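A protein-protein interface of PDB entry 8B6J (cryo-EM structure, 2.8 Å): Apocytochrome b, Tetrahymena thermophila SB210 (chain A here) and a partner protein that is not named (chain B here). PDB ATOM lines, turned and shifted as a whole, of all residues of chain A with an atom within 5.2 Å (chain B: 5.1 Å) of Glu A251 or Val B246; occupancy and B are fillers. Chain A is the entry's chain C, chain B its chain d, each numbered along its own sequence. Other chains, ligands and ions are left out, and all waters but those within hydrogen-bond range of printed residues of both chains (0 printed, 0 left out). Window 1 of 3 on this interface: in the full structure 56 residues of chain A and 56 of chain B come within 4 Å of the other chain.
The side-chain carboxylate of Glu A251 lies within salt-bridge range of the guanidinium group of Arg B250, 3.5 Å away.
CE2 of Phe B59 touches CG of Glu A251, 3.5 Å away. Glu A251 touches Val B246 (OE2 to CG1, 3.4 Å). CG of Pro A252 touches CD2 of Phe B59, at 3.7 Å.
Of chain B, only Phe B59 (3.5 Å), Val B246 (3.4 Å) and Arg B250 (3.1 Å) come within 4 Å of Glu A251. Val B246 touches one residue of chain A. Of the printed residues of chain A, Arg B250 touches Glu A251 (3.1 Å). Printed residues of chain A within 4 Å of Phe B59: Glu A251 (3.5 Å) and Pro A252 (3.7 Å). Of the printed residues of chain B, Pro A252 touches Phe B59. Glu A253 touches none of the printed residues of chain B. The nearest residue of chain B that does not touch Glu A251 is Arg B245 (4.7 Å). The nearest printed residue of chain A that does not touch Arg B250 is Pro A252 (5.2 Å).
Of the 5 printed residues of chain A, 2 touch a printed residue of chain B. Hydrophobic or aromatic side chains of chain A that line the printed part of chain B: Pro A252. Of the 11 printed residues of chain B, 3 touch a printed residue of chain A. Hydrophobic or aromatic side chains of chain B within 4 Å of the printed part of chain A: Phe B59 and Val B246.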
ATOM      1  N   TYR A 249     -27.893   4.959  -4.741  1.00  0.00           N
ATOM      2  CA  TYR A 249     -26.988   3.826  -4.546  1.00  0.00           C
ATOM      3  C   TYR A 249     -27.624   2.793  -3.625  1.00  0.00           C
ATOM      4  O   TYR A 249     -27.222   2.647  -2.464  1.00  0.00           O
ATOM      5  CB  TYR A 249     -25.647   4.288  -3.973  1.00  0.00           C
ATOM      6  CG  TYR A 249     -24.784   5.058  -4.944  1.00  0.00           C
ATOM      7  CD1 TYR A 249     -24.033   4.398  -5.905  1.00  0.00           C
ATOM      8  CD2 TYR A 249     -24.711   6.442  -4.891  1.00  0.00           C
ATOM      9  CE1 TYR A 249     -23.239   5.095  -6.789  1.00  0.00           C
ATOM     10  CE2 TYR A 249     -23.920   7.147  -5.773  1.00  0.00           C
ATOM     11  CZ  TYR A 249     -23.186   6.469  -6.720  1.00  0.00           C
ATOM     12  OH  TYR A 249     -22.394   7.165  -7.602  1.00  0.00           O
ATOM     13  N   PRO A 250     -28.620   2.054  -4.109  1.00  0.00           N
ATOM     14  CA  PRO A 250     -29.063   0.869  -3.368  1.00  0.00           C
ATOM     15  C   PRO A 250     -27.925  -0.134  -3.274  1.00  0.00           C
ATOM     16  O   PRO A 250     -27.189  -0.351  -4.239  1.00  0.00           O
ATOM     17  CB  PRO A 250     -30.231   0.338  -4.206  1.00  0.00           C
ATOM     18  CG  PRO A 250     -30.003   0.886  -5.571  1.00  0.00           C
ATOM     19  CD  PRO A 250     -29.357   2.222  -5.372  1.00  0.00           C
ATOM     20  N   GLU A 251     -27.777  -0.746  -2.101  1.00  0.00           N
ATOM     21  CA  GLU A 251     -26.611  -1.597  -1.877  1.00  0.00           C
ATOM     22  C   GLU A 251     -26.540  -2.746  -2.871  1.00  0.00           C
ATOM     23  O   GLU A 251     -25.470  -2.948  -3.471  1.00  0.00           O
ATOM     24  CB  GLU A 251     -26.603  -2.106  -0.433  1.00  0.00           C
ATOM     25  CG  GLU A 251     -25.258  -2.663   0.013  1.00  0.00           C
ATOM     26  CD  GLU A 251     -24.224  -1.578   0.260  1.00  0.00           C
ATOM     27  OE1 GLU A 251     -24.466  -0.418  -0.138  1.00  0.00           O
ATOM     28  OE2 GLU A 251     -23.170  -1.884   0.856  1.00  0.00           O
ATOM     29  N   PRO A 252     -27.601  -3.529  -3.099  1.00  0.00           N
ATOM     30  CA  PRO A 252     -27.569  -4.515  -4.186  1.00  0.00           C
ATOM     31  C   PRO A 252     -27.864  -3.843  -5.516  1.00  0.00           C
ATOM     32  O   PRO A 252     -29.006  -3.471  -5.802  1.00  0.00           O
ATOM     33  CB  PRO A 252     -28.665  -5.512  -3.782  1.00  0.00           C
ATOM     34  CG  PRO A 252     -29.569  -4.763  -2.825  1.00  0.00           C
ATOM     35  CD  PRO A 252     -28.945  -3.430  -2.507  1.00  0.00           C
ATOM     36  N   GLU A 253     -26.829  -3.683  -6.336  1.00  0.00           N
ATOM     37  CA  GLU A 253     -26.927  -2.973  -7.601  1.00  0.00           C
ATOM     38  C   GLU A 253     -26.463  -3.882  -8.729  1.00  0.00           C
ATOM     39  O   GLU A 253     -25.505  -4.644  -8.568  1.00  0.00           O
ATOM     40  CB  GLU A 253     -26.091  -1.691  -7.578  1.00  0.00           C
ATOM     41  CG  GLU A 253     -26.284  -0.803  -8.796  1.00  0.00           C
ATOM     42  CD  GLU A 253     -25.552   0.521  -8.676  1.00  0.00           C
ATOM     43  OE1 GLU A 253     -25.161   0.885  -7.547  1.00  0.00           O
ATOM     44  OE2 GLU A 253     -25.365   1.197  -9.710  1.00  0.00           O
ATOM     45  N   PHE B  59     -30.676  -7.133   3.172  1.00  0.00           N
ATOM     46  CA  PHE B  59     -30.789  -5.836   2.519  1.00  0.00           C
ATOM     47  C   PHE B  59     -32.162  -5.200   2.687  1.00  0.00           C
ATOM     48  O   PHE B  59     -32.364  -4.072   2.228  1.00  0.00           O
ATOM     49  CB  PHE B  59     -30.461  -5.973   1.030  1.00  0.00           C
ATOM     50  CG  PHE B  59     -29.040  -6.370   0.765  1.00  0.00           C
ATOM     51  CD1 PHE B  59     -28.666  -7.702   0.777  1.00  0.00           C
ATOM     52  CD2 PHE B  59     -28.076  -5.412   0.513  1.00  0.00           C
ATOM     53  CE1 PHE B  59     -27.358  -8.069   0.538  1.00  0.00           C
ATOM     54  CE2 PHE B  59     -26.766  -5.774   0.273  1.00  0.00           C
ATOM     55  CZ  PHE B  59     -26.407  -7.103   0.286  1.00  0.00           C
ATOM     56  N   LYS B 166     -18.152 -10.389  -3.801  1.00  0.00           N
ATOM     57  CA  LYS B 166     -19.274  -9.456  -3.815  1.00  0.00           C
ATOM     58  C   LYS B 166     -19.243  -8.552  -5.038  1.00  0.00           C
ATOM     59  O   LYS B 166     -20.289  -8.061  -5.473  1.00  0.00           O
ATOM     60  CB  LYS B 166     -19.256  -8.609  -2.546  1.00  0.00           C
ATOM     61  CG  LYS B 166     -17.935  -7.894  -2.317  1.00  0.00           C
ATOM     62  CD  LYS B 166     -18.021  -6.883  -1.194  1.00  0.00           C
ATOM     63  CE  LYS B 166     -16.667  -6.254  -0.924  1.00  0.00           C
ATOM     64  NZ  LYS B 166     -16.726  -5.261   0.180  1.00  0.00           N
ATOM     65  N   ASN B 240     -22.329 -14.230   1.104  1.00  0.00           N
ATOM     66  CA  ASN B 240     -22.447 -12.801   1.369  1.00  0.00           C
ATOM     67  C   ASN B 240     -22.108 -12.469   2.817  1.00  0.00           C
ATOM     68  O   ASN B 240     -21.642 -11.361   3.104  1.00  0.00           O
ATOM     69  CB  ASN B 240     -23.856 -12.320   1.028  1.00  0.00           C
ATOM     70  CG  ASN B 240     -24.047 -10.844   1.298  1.00  0.00           C
ATOM     71  OD1 ASN B 240     -24.610 -10.457   2.319  1.00  0.00           O
ATOM     72  ND2 ASN B 240     -23.575 -10.009   0.382  1.00  0.00           N
ATOM     73  N   MET B 242     -19.691 -13.377   4.526  1.00  0.00           N
ATOM     74  CA  MET B 242     -18.254 -13.292   4.749  1.00  0.00           C
ATOM     75  C   MET B 242     -17.627 -12.030   4.173  1.00  0.00           C
ATOM     76  O   MET B 242     -16.432 -11.802   4.384  1.00  0.00           O
ATOM     77  CB  MET B 242     -17.564 -14.518   4.144  1.00  0.00           C
ATOM     78  CG  MET B 242     -18.201 -15.841   4.530  1.00  0.00           C
ATOM     79  SD  MET B 242     -18.114 -16.194   6.293  1.00  0.00           S
ATOM     80  CE  MET B 242     -16.369 -16.541   6.479  1.00  0.00           C
ATOM     81  N   GLN B 243     -18.390 -11.209   3.458  1.00  0.00           N
ATOM     82  CA  GLN B 243     -17.853  -9.996   2.864  1.00  0.00           C
ATOM     83  C   GLN B 243     -17.649  -8.928   3.937  1.00  0.00           C
ATOM     84  O   GLN B 243     -18.168  -9.028   5.051  1.00  0.00           O
ATOM     85  CB  GLN B 243     -18.787  -9.489   1.767  1.00  0.00           C
ATOM     86  CG  GLN B 243     -19.252 -10.574   0.803  1.00  0.00           C
ATOM     87  CD  GLN B 243     -18.106 -11.238   0.068  1.00  0.00           C
ATOM     88  OE1 GLN B 243     -17.122 -10.591  -0.281  1.00  0.00           O
ATOM     89  NE2 GLN B 243     -18.228 -12.538  -0.167  1.00  0.00           N
ATOM     90  N   ARG B 244     -16.880  -7.892   3.594  1.00  0.00           N
ATOM     91  CA  ARG B 244     -16.480  -6.908   4.599  1.00  0.00           C
ATOM     92  C   ARG B 244     -17.436  -5.716   4.661  1.00  0.00           C
ATOM     93  O   ARG B 244     -18.023  -5.446   5.714  1.00  0.00           O
ATOM     94  CB  ARG B 244     -15.035  -6.447   4.349  1.00  0.00           C
ATOM     95  CG  ARG B 244     -14.755  -5.805   3.000  1.00  0.00           C
ATOM     96  CD  ARG B 244     -13.287  -5.443   2.864  1.00  0.00           C
ATOM     97  NE  ARG B 244     -13.006  -4.766   1.605  1.00  0.00           N
ATOM     98  CZ  ARG B 244     -13.167  -3.466   1.400  1.00  0.00           C
ATOM     99  NH1 ARG B 244     -13.610  -2.664   2.353  1.00  0.00           N
ATOM    100  NH2 ARG B 244     -12.878  -2.958   0.206  1.00  0.00           N
ATOM    101  N   ARG B 245     -17.604  -4.990   3.553  1.00  0.00           N
ATOM    102  CA  ARG B 245     -18.517  -3.850   3.563  1.00  0.00           C
ATOM    103  C   ARG B 245     -19.962  -4.320   3.589  1.00  0.00           C
ATOM    104  O   ARG B 245     -20.780  -3.814   4.366  1.00  0.00           O
ATOM    105  CB  ARG B 245     -18.266  -2.955   2.352  1.00  0.00           C
ATOM    106  CG  ARG B 245     -17.014  -2.114   2.457  1.00  0.00           C
ATOM    107  CD  ARG B 245     -17.148  -1.032   3.514  1.00  0.00           C
ATOM    108  NE  ARG B 245     -15.900  -0.299   3.683  1.00  0.00           N
ATOM    109  CZ  ARG B 245     -15.518   0.720   2.928  1.00  0.00           C
ATOM    110  NH1 ARG B 245     -16.277   1.177   1.946  1.00  0.00           N
ATOM    111  NH2 ARG B 245     -14.341   1.292   3.159  1.00  0.00           N
ATOM    112  N   VAL B 246     -20.292  -5.283   2.744  1.00  0.00           N
ATOM    113  CA  VAL B 246     -21.562  -5.981   2.829  1.00  0.00           C
ATOM    114  C   VAL B 246     -21.355  -7.227   3.680  1.00  0.00           C
ATOM    115  O   VAL B 246     -20.230  -7.686   3.888  1.00  0.00           O
ATOM    116  CB  VAL B 246     -22.108  -6.336   1.431  1.00  0.00           C
ATOM    117  CG1 VAL B 246     -22.183  -5.092   0.561  1.00  0.00           C
ATOM    118  CG2 VAL B 246     -21.247  -7.400   0.773  1.00  0.00           C
ATOM    119  N   GLY B 247     -22.448  -7.767   4.203  1.00  0.00           N
ATOM    120  CA  GLY B 247     -22.359  -8.983   4.985  1.00  0.00           C
ATOM    121  C   GLY B 247     -22.642  -8.792   6.460  1.00  0.00           C
ATOM    122  O   GLY B 247     -23.560  -8.058   6.838  1.00  0.00           O
ATOM    123  N   TYR B 248     -21.848  -9.451   7.304  1.00  0.00           N
ATOM    124  CA  TYR B 248     -22.171  -9.541   8.722  1.00  0.00           C
ATOM    125  C   TYR B 248     -22.191  -8.185   9.413  1.00  0.00           C
ATOM    126  O   TYR B 248     -22.784  -8.066  10.490  1.00  0.00           O
ATOM    127  CB  TYR B 248     -21.178 -10.471   9.422  1.00  0.00           C
ATOM    128  CG  TYR B 248     -19.749  -9.978   9.423  1.00  0.00           C
ATOM    129  CD1 TYR B 248     -18.939 -10.135   8.307  1.00  0.00           C
ATOM    130  CD2 TYR B 248     -19.205  -9.368  10.545  1.00  0.00           C
ATOM    131  CE1 TYR B 248     -17.636  -9.690   8.303  1.00  0.00           C
ATOM    132  CE2 TYR B 248     -17.901  -8.922  10.550  1.00  0.00           C
ATOM    133  CZ  TYR B 248     -17.122  -9.085   9.427  1.00  0.00           C
ATOM    134  OH  TYR B 248     -15.821  -8.641   9.425  1.00  0.00           O
ATOM    135  N   ARG B 250     -22.980  -5.091   7.631  1.00  0.00           N
ATOM    136  CA  ARG B 250     -23.794  -4.082   6.956  1.00  0.00           C
ATOM    137  C   ARG B 250     -25.040  -3.698   7.741  1.00  0.00           C
ATOM    138  O   ARG B 250     -25.297  -2.492   7.889  1.00  0.00           O
ATOM    139  CB  ARG B 250     -24.168  -4.567   5.553  1.00  0.00           C
ATOM    140  CG  ARG B 250     -25.374  -3.841   4.983  1.00  0.00           C
ATOM    141  CD  ARG B 250     -25.578  -4.107   3.510  1.00  0.00           C
ATOM    142  NE  ARG B 250     -26.836  -3.532   3.048  1.00  0.00           N
ATOM    143  CZ  ARG B 250     -27.011  -2.254   2.743  1.00  0.00           C
ATOM    144  NH1 ARG B 250     -26.020  -1.381   2.820  1.00  0.00           N
ATOM    145  NH2 ARG B 250     -28.211  -1.840   2.347  1.00  0.00           N
